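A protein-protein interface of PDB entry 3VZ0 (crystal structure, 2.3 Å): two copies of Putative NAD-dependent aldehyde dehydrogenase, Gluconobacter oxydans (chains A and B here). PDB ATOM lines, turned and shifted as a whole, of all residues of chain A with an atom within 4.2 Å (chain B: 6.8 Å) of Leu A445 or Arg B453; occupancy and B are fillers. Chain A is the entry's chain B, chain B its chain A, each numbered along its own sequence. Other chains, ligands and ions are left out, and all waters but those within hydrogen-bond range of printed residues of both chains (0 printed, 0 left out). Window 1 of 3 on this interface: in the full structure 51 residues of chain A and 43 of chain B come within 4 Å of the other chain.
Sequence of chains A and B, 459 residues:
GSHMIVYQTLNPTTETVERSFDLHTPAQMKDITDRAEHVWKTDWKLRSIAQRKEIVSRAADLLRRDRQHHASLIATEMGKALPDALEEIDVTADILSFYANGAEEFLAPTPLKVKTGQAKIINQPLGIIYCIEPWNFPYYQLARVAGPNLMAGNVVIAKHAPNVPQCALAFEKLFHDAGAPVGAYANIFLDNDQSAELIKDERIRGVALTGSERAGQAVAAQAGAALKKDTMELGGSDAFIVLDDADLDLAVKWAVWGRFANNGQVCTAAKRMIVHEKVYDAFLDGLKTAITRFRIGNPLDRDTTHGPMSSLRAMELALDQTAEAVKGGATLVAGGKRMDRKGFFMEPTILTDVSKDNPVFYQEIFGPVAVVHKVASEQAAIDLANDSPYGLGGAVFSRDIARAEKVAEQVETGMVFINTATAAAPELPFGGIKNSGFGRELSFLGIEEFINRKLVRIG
Arg B453 touches three residues of chain A.
Printed residues of chain B within 4 Å of Arg A440: Asn B452 and Arg B453.
Of the printed residues of chain A, Leu B455 touches Gly A414.
Of the printed residues of chain A, Lys B454 touches Gly A414 (3.3 Å).
Of the printed residues of chain B, Gly A414 touches Asn B452 (3.8 Å), Arg B453 (3.7 Å), Lys B454 (3.3 Å) and Leu B455 (3.0 Å).
Printed residues of chain A within 4 Å of Asn B452: Gly A414 and Arg A440.
Glu B448 touches none of the printed residues of chain A.
The nearest residue of chain B that does not touch Leu A445 is Ile B121 (4.1 Å).
The nearest printed residue of chain A that does not touch Lys B454 is Arg A440 (4.3 Å).
Of the 10 printed residues of chain A, 3 touch a printed residue of chain B.
Among the printed residues, 7 pairs touch across the chains.
Among the printed residues, no Asp or Glu carboxylate lies within 4 Å of a Lys or Arg side-chain nitrogen of the other chain.
The side-chain amino group of Lys B454 lies within hydrogen-bond range of the side-chain amide oxygen of Gln B124, 2.9 Å away.
N of Leu A445 lies close to OG of Ser A443 (3.2 Å).
The backbone NH (N) of Arg A440 lies within hydrogen-bond range of the side-chain carboxylate (OE2) of Glu A449 (3.2 Å).
The backbone carbonyl oxygen (O) of Lys B454 lies within hydrogen-bond range of the backbone NH (N) of Ile B122, 2.8 Å away.
OE1 of Glu B448 is in salt-bridge range of NH1 of Arg B453 (3.4 Å).
The backbone carbonyl oxygen (O) of Gln B124 is in hydrogen-bond range of the backbone NH (N) of Asn B452 (2.8 Å).
Positions printed for both chains: 445, 448 and 449.
CA of Gly A414 touches OD1 of Asn B452, at 3.8 Å.
Arg B453 touches Gly A414.
Gly A414 touches Lys B454 (O to CA, 3.3 Å).
Arg B453 touches Leu A445.
The guanidinium group (NH1) of Arg A440 lies within hydrogen-bond range of the backbone carbonyl oxygen (O) of Arg B453, 2.5 Å away.
OD1 of Asn B452 sits at hydrogen-bond distance from NH1 of Arg A440 (3.4 Å).
The backbone NH (N) of Leu B455 lies within hydrogen-bond range of the backbone carbonyl oxygen (O) of Gly A414, 3.0 Å away.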
ATOM      1  N   GLY A 414       2.106  -0.873  -7.756  1.00  0.00           N
ATOM      2  CA  GLY A 414       1.243  -0.853  -6.580  1.00  0.00           C
ATOM      3  C   GLY A 414       1.889  -0.291  -5.318  1.00  0.00           C
ATOM      4  O   GLY A 414       1.197   0.190  -4.428  1.00  0.00           O
ATOM      5  N   ARG A 440      -5.572  -5.539  -2.478  1.00  0.00           N
ATOM      6  CA  ARG A 440      -4.575  -5.304  -1.424  1.00  0.00           C
ATOM      7  C   ARG A 440      -4.798  -6.251  -0.240  1.00  0.00           C
ATOM      8  O   ARG A 440      -5.900  -6.300   0.315  1.00  0.00           O
ATOM      9  CB  ARG A 440      -4.643  -3.853  -0.902  1.00  0.00           C
ATOM     10  CG  ARG A 440      -4.529  -2.723  -1.939  1.00  0.00           C
ATOM     11  CD  ARG A 440      -3.103  -2.543  -2.490  1.00  0.00           C
ATOM     12  NE  ARG A 440      -2.998  -3.019  -3.871  1.00  0.00           N
ATOM     13  CZ  ARG A 440      -2.782  -2.247  -4.934  1.00  0.00           C
ATOM     14  NH1 ARG A 440      -2.617  -0.938  -4.805  1.00  0.00           N
ATOM     15  NH2 ARG A 440      -2.718  -2.796  -6.138  1.00  0.00           N
ATOM     16  N   LEU A 442      -2.786  -7.400   3.711  1.00  0.00           N
ATOM     17  CA  LEU A 442      -2.135  -6.721   4.845  1.00  0.00           C
ATOM     18  C   LEU A 442      -2.786  -5.368   5.175  1.00  0.00           C
ATOM     19  O   LEU A 442      -3.612  -4.868   4.404  1.00  0.00           O
ATOM     20  CB  LEU A 442      -0.606  -6.614   4.674  1.00  0.00           C
ATOM     21  CG  LEU A 442       0.184  -7.915   4.458  1.00  0.00           C
ATOM     22  CD1 LEU A 442       1.686  -7.678   4.511  1.00  0.00           C
ATOM     23  CD2 LEU A 442      -0.222  -8.967   5.473  1.00  0.00           C
ATOM     24  N   SER A 443      -2.415  -4.806   6.330  1.00  0.00           N
ATOM     25  CA  SER A 443      -3.058  -3.609   6.939  1.00  0.00           C
ATOM     26  C   SER A 443      -4.586  -3.754   7.125  1.00  0.00           C
ATOM     27  O   SER A 443      -5.133  -4.871   7.058  1.00  0.00           O
ATOM     28  CB  SER A 443      -2.697  -2.311   6.183  1.00  0.00           C
ATOM     29  OG  SER A 443      -3.626  -2.023   5.151  1.00  0.00           O
ATOM     30  N   PHE A 444      -5.259  -2.627   7.364  1.00  0.00           N
ATOM     31  CA  PHE A 444      -6.729  -2.573   7.434  1.00  0.00           C
ATOM     32  C   PHE A 444      -7.421  -2.973   6.113  1.00  0.00           C
ATOM     33  O   PHE A 444      -8.605  -3.324   6.109  1.00  0.00           O
ATOM     34  CB  PHE A 444      -7.207  -1.179   7.902  1.00  0.00           C
ATOM     35  CG  PHE A 444      -6.937  -0.069   6.908  1.00  0.00           C
ATOM     36  CD1 PHE A 444      -7.929   0.336   6.011  1.00  0.00           C
ATOM     37  CD2 PHE A 444      -5.693   0.567   6.868  1.00  0.00           C
ATOM     38  CE1 PHE A 444      -7.683   1.357   5.084  1.00  0.00           C
ATOM     39  CE2 PHE A 444      -5.438   1.589   5.949  1.00  0.00           C
ATOM     40  CZ  PHE A 444      -6.434   1.986   5.055  1.00  0.00           C
ATOM     41  N   LEU A 445      -6.681  -2.906   5.002  1.00  0.00           N
ATOM     42  CA  LEU A 445      -7.213  -3.268   3.685  1.00  0.00           C
ATOM     43  C   LEU A 445      -7.362  -4.783   3.447  1.00  0.00           C
ATOM     44  O   LEU A 445      -8.264  -5.213   2.710  1.00  0.00           O
ATOM     45  CB  LEU A 445      -6.372  -2.638   2.562  1.00  0.00           C
ATOM     46  CG  LEU A 445      -6.608  -1.157   2.222  1.00  0.00           C
ATOM     47  CD1 LEU A 445      -5.746  -0.737   1.040  1.00  0.00           C
ATOM     48  CD2 LEU A 445      -8.094  -0.861   1.953  1.00  0.00           C
ATOM     49  N   GLY A 446      -6.482  -5.576   4.064  1.00  0.00           N
ATOM     50  CA  GLY A 446      -6.471  -7.032   3.867  1.00  0.00           C
ATOM     51  C   GLY A 446      -7.665  -7.751   4.468  1.00  0.00           C
ATOM     52  O   GLY A 446      -8.110  -8.794   3.961  1.00  0.00           O
ATOM     53  N   ILE A 447      -8.188  -7.185   5.552  1.00  0.00           N
ATOM     54  CA  ILE A 447      -9.296  -7.786   6.286  1.00  0.00           C
ATOM     55  C   ILE A 447     -10.643  -7.497   5.616  1.00  0.00           C
ATOM     56  O   ILE A 447     -11.662  -8.074   5.995  1.00  0.00           O
ATOM     57  CB  ILE A 447      -9.285  -7.362   7.795  1.00  0.00           C
ATOM     58  CG1 ILE A 447      -9.939  -8.455   8.663  1.00  0.00           C
ATOM     59  CG2 ILE A 447      -9.901  -5.969   7.993  1.00  0.00           C
ATOM     60  CD1 ILE A 447      -9.564  -8.429  10.126  1.00  0.00           C
ATOM     61  N   GLU A 448     -10.626  -6.631   4.602  1.00  0.00           N
ATOM     62  CA  GLU A 448     -11.845  -6.138   3.958  1.00  0.00           C
ATOM     63  C   GLU A 448     -12.155  -6.816   2.637  1.00  0.00           C
ATOM     64  O   GLU A 448     -13.190  -6.537   2.031  1.00  0.00           O
ATOM     65  CB  GLU A 448     -11.774  -4.620   3.741  1.00  0.00           C
ATOM     66  CG  GLU A 448     -11.573  -3.842   5.019  1.00  0.00           C
ATOM     67  CD  GLU A 448     -11.611  -2.349   4.815  1.00  0.00           C
ATOM     68  OE1 GLU A 448     -11.257  -1.875   3.703  1.00  0.00           O
ATOM     69  OE2 GLU A 448     -11.994  -1.649   5.781  1.00  0.00           O
ATOM     70  N   GLU A 449     -11.266  -7.697   2.193  1.00  0.00           N
ATOM     71  CA  GLU A 449     -11.439  -8.362   0.899  1.00  0.00           C
ATOM     72  C   GLU A 449     -12.654  -9.284   0.881  1.00  0.00           C
ATOM     73  O   GLU A 449     -13.488  -9.179  -0.024  1.00  0.00           O
ATOM     74  CB  GLU A 449     -10.169  -9.123   0.482  1.00  0.00           C
ATOM     75  CG  GLU A 449      -9.034  -8.239  -0.041  1.00  0.00           C
ATOM     76  CD  GLU A 449      -9.342  -7.561  -1.395  1.00  0.00           C
ATOM     77  OE1 GLU A 449     -10.511  -7.534  -1.829  1.00  0.00           O
ATOM     78  OE2 GLU A 449      -8.402  -7.047  -2.037  1.00  0.00           O
ATOM     79  N   ILE B 121      -0.953   6.271   1.113  1.00  0.00           N
ATOM     80  CA  ILE B 121      -1.580   5.714  -0.071  1.00  0.00           C
ATOM     81  C   ILE B 121      -1.970   6.857  -1.013  1.00  0.00           C
ATOM     82  O   ILE B 121      -2.680   7.774  -0.623  1.00  0.00           O
ATOM     83  CB  ILE B 121      -2.820   4.876   0.285  1.00  0.00           C
ATOM     84  CG1 ILE B 121      -2.409   3.646   1.098  1.00  0.00           C
ATOM     85  CG2 ILE B 121      -3.568   4.487  -0.971  1.00  0.00           C
ATOM     86  CD1 ILE B 121      -3.586   2.762   1.509  1.00  0.00           C
ATOM     87  N   ILE B 122      -1.458   6.817  -2.235  1.00  0.00           N
ATOM     88  CA  ILE B 122      -1.745   7.842  -3.228  1.00  0.00           C
ATOM     89  C   ILE B 122      -2.776   7.262  -4.190  1.00  0.00           C
ATOM     90  O   ILE B 122      -2.616   6.137  -4.669  1.00  0.00           O
ATOM     91  CB  ILE B 122      -0.436   8.275  -3.967  1.00  0.00           C
ATOM     92  CG1 ILE B 122       0.551   8.928  -2.989  1.00  0.00           C
ATOM     93  CG2 ILE B 122      -0.724   9.207  -5.120  1.00  0.00           C
ATOM     94  CD1 ILE B 122       0.070  10.218  -2.389  1.00  0.00           C
ATOM     95  N   ASN B 123      -3.834   8.012  -4.472  1.00  0.00           N
ATOM     96  CA  ASN B 123      -4.888   7.494  -5.330  1.00  0.00           C
ATOM     97  C   ASN B 123      -4.690   7.930  -6.789  1.00  0.00           C
ATOM     98  O   ASN B 123      -4.758   9.114  -7.129  1.00  0.00           O
ATOM     99  CB  ASN B 123      -6.272   7.879  -4.789  1.00  0.00           C
ATOM    100  CG  ASN B 123      -6.471   7.435  -3.346  1.00  0.00           C
ATOM    101  OD1 ASN B 123      -6.597   6.250  -3.068  1.00  0.00           O
ATOM    102  ND2 ASN B 123      -6.481   8.392  -2.420  1.00  0.00           N
ATOM    103  N   GLN B 124      -4.422   6.962  -7.647  1.00  0.00           N
ATOM    104  CA  GLN B 124      -4.186   7.250  -9.044  1.00  0.00           C
ATOM    105  C   GLN B 124      -5.170   6.499  -9.970  1.00  0.00           C
ATOM    106  O   GLN B 124      -5.641   5.413  -9.631  1.00  0.00           O
ATOM    107  CB  GLN B 124      -2.724   6.961  -9.369  1.00  0.00           C
ATOM    108  CG  GLN B 124      -1.777   7.946  -8.673  1.00  0.00           C
ATOM    109  CD  GLN B 124      -0.316   7.668  -8.931  1.00  0.00           C
ATOM    110  OE1 GLN B 124       0.093   6.517  -9.082  1.00  0.00           O
ATOM    111  NE2 GLN B 124       0.491   8.729  -8.964  1.00  0.00           N
ATOM    112  N   LEU B 126      -6.586   4.284 -13.198  1.00  0.00           N
ATOM    113  CA  LEU B 126      -6.149   3.032 -13.802  1.00  0.00           C
ATOM    114  C   LEU B 126      -6.081   3.143 -15.316  1.00  0.00           C
ATOM    115  O   LEU B 126      -5.130   2.669 -15.937  1.00  0.00           O
ATOM    116  CB  LEU B 126      -7.136   1.920 -13.447  1.00  0.00           C
ATOM    117  CG  LEU B 126      -6.603   0.642 -12.830  1.00  0.00           C
ATOM    118  CD1 LEU B 126      -5.293   0.830 -12.077  1.00  0.00           C
ATOM    119  CD2 LEU B 126      -7.661   0.131 -11.894  1.00  0.00           C
ATOM    120  N   LYS B 229      -9.666  -6.296 -12.912  1.00  0.00           N
ATOM    121  CA  LYS B 229     -10.603  -5.897 -11.886  1.00  0.00           C
ATOM    122  C   LYS B 229     -12.015  -5.812 -12.511  1.00  0.00           C
ATOM    123  O   LYS B 229     -12.184  -5.424 -13.663  1.00  0.00           O
ATOM    124  CB  LYS B 229     -10.182  -4.553 -11.271  1.00  0.00           C
ATOM    125  CG  LYS B 229      -8.663  -4.306 -11.279  1.00  0.00           C
ATOM    126  CD  LYS B 229      -8.165  -3.427 -10.107  1.00  0.00           C
ATOM    127  CE  LYS B 229      -6.667  -3.064 -10.322  1.00  0.00           C
ATOM    128  NZ  LYS B 229      -5.895  -2.619  -9.107  1.00  0.00           N
ATOM    129  N   LEU B 445     -17.162   4.397  -1.093  1.00  0.00           N
ATOM    130  CA  LEU B 445     -16.738   3.059  -1.496  1.00  0.00           C
ATOM    131  C   LEU B 445     -16.738   2.873  -3.028  1.00  0.00           C
ATOM    132  O   LEU B 445     -15.803   2.283  -3.584  1.00  0.00           O
ATOM    133  CB  LEU B 445     -17.612   2.013  -0.804  1.00  0.00           C
ATOM    134  CG  LEU B 445     -17.028   0.705  -0.268  1.00  0.00           C
ATOM    135  CD1 LEU B 445     -15.619   0.861   0.332  1.00  0.00           C
ATOM    136  CD2 LEU B 445     -18.001   0.131   0.764  1.00  0.00           C
ATOM    137  N   GLU B 448     -13.451   3.772  -4.896  1.00  0.00           N
ATOM    138  CA  GLU B 448     -12.293   2.904  -4.595  1.00  0.00           C
ATOM    139  C   GLU B 448     -12.079   1.758  -5.603  1.00  0.00           C
ATOM    140  O   GLU B 448     -10.966   1.229  -5.724  1.00  0.00           O
ATOM    141  CB  GLU B 448     -12.432   2.280  -3.192  1.00  0.00           C
ATOM    142  CG  GLU B 448     -12.321   3.241  -1.979  1.00  0.00           C
ATOM    143  CD  GLU B 448     -12.463   2.513  -0.602  1.00  0.00           C
ATOM    144  OE1 GLU B 448     -12.392   1.250  -0.544  1.00  0.00           O
ATOM    145  OE2 GLU B 448     -12.636   3.211   0.432  1.00  0.00           O
ATOM    146  N   GLU B 449     -13.140   1.374  -6.312  1.00  0.00           N
ATOM    147  CA  GLU B 449     -13.153   0.124  -7.092  1.00  0.00           C
ATOM    148  C   GLU B 449     -12.073   0.019  -8.187  1.00  0.00           C
ATOM    149  O   GLU B 449     -11.418  -1.020  -8.325  1.00  0.00           O
ATOM    150  CB  GLU B 449     -14.539  -0.108  -7.717  1.00  0.00           C
ATOM    151  CG  GLU B 449     -15.699  -0.228  -6.724  1.00  0.00           C
ATOM    152  CD  GLU B 449     -17.062  -0.107  -7.403  1.00  0.00           C
ATOM    153  OE1 GLU B 449     -17.319   0.934  -8.072  1.00  0.00           O
ATOM    154  OE2 GLU B 449     -17.886  -1.052  -7.252  1.00  0.00           O
ATOM    155  N   ILE B 451      -9.200   2.200  -8.938  1.00  0.00           N
ATOM    156  CA  ILE B 451      -8.048   3.076  -8.817  1.00  0.00           C
ATOM    157  C   ILE B 451      -6.827   2.267  -8.413  1.00  0.00           C
ATOM    158  O   ILE B 451      -6.965   1.183  -7.831  1.00  0.00           O
ATOM    159  CB  ILE B 451      -8.303   4.232  -7.799  1.00  0.00           C
ATOM    160  CG1 ILE B 451      -8.701   3.677  -6.426  1.00  0.00           C
ATOM    161  CG2 ILE B 451      -9.359   5.210  -8.343  1.00  0.00           C
ATOM    162  CD1 ILE B 451      -8.779   4.737  -5.323  1.00  0.00           C
ATOM    163  N   ASN B 452      -5.639   2.769  -8.741  1.00  0.00           N
ATOM    164  CA  ASN B 452      -4.419   2.241  -8.118  1.00  0.00           C
ATOM    165  C   ASN B 452      -4.199   2.948  -6.783  1.00  0.00           C
ATOM    166  O   ASN B 452      -3.880   4.134  -6.729  1.00  0.00           O
ATOM    167  CB  ASN B 452      -3.186   2.380  -9.031  1.00  0.00           C
ATOM    168  CG  ASN B 452      -1.875   1.872  -8.368  1.00  0.00           C
ATOM    169  OD1 ASN B 452      -1.895   1.080  -7.414  1.00  0.00           O
ATOM    170  ND2 ASN B 452      -0.737   2.325  -8.892  1.00  0.00           N
ATOM    171  N   ARG B 453      -4.417   2.214  -5.704  1.00  0.00           N
ATOM    172  CA  ARG B 453      -4.051   2.686  -4.390  1.00  0.00           C
ATOM    173  C   ARG B 453      -2.592   2.340  -4.138  1.00  0.00           C
ATOM    174  O   ARG B 453      -2.242   1.242  -3.685  1.00  0.00           O
ATOM    175  CB  ARG B 453      -4.999   2.101  -3.349  1.00  0.00           C
ATOM    176  CG  ARG B 453      -6.381   2.731  -3.439  1.00  0.00           C
ATOM    177  CD  ARG B 453      -7.285   2.211  -2.368  1.00  0.00           C
ATOM    178  NE  ARG B 453      -7.592   0.798  -2.586  1.00  0.00           N
ATOM    179  CZ  ARG B 453      -8.449   0.100  -1.847  1.00  0.00           C
ATOM    180  NH1 ARG B 453      -9.088   0.686  -0.837  1.00  0.00           N
ATOM    181  NH2 ARG B 453      -8.672  -1.184  -2.124  1.00  0.00           N
ATOM    182  N   LYS B 454      -1.738   3.296  -4.486  1.00  0.00           N
ATOM    183  CA  LYS B 454      -0.309   3.124  -4.453  1.00  0.00           C
ATOM    184  C   LYS B 454       0.226   3.430  -3.064  1.00  0.00           C
ATOM    185  O   LYS B 454       0.063   4.548  -2.565  1.00  0.00           O
ATOM    186  CB  LYS B 454       0.343   4.029  -5.505  1.00  0.00           C
ATOM    187  CG  LYS B 454       1.852   3.989  -5.511  1.00  0.00           C
ATOM    188  CD  LYS B 454       2.463   5.066  -6.409  1.00  0.00           C
ATOM    189  CE  LYS B 454       2.604   4.593  -7.842  1.00  0.00           C
ATOM    190  NZ  LYS B 454       2.869   5.703  -8.828  1.00  0.00           N
ATOM    191  N   LEU B 455       0.862   2.425  -2.450  1.00  0.00           N
ATOM    192  CA  LEU B 455       1.649   2.626  -1.232  1.00  0.00           C
ATOM    193  C   LEU B 455       2.968   3.288  -1.584  1.00  0.00           C
ATOM    194  O   LEU B 455       3.705   2.812  -2.456  1.00  0.00           O
ATOM    195  CB  LEU B 455       1.908   1.310  -0.482  1.00  0.00           C
ATOM    196  CG  LEU B 455       2.940   1.399   0.669  1.00  0.00           C
ATOM    197  CD1 LEU B 455       2.371   2.103   1.924  1.00  0.00           C
ATOM    198  CD2 LEU B 455       3.552   0.036   1.022  1.00  0.00           C
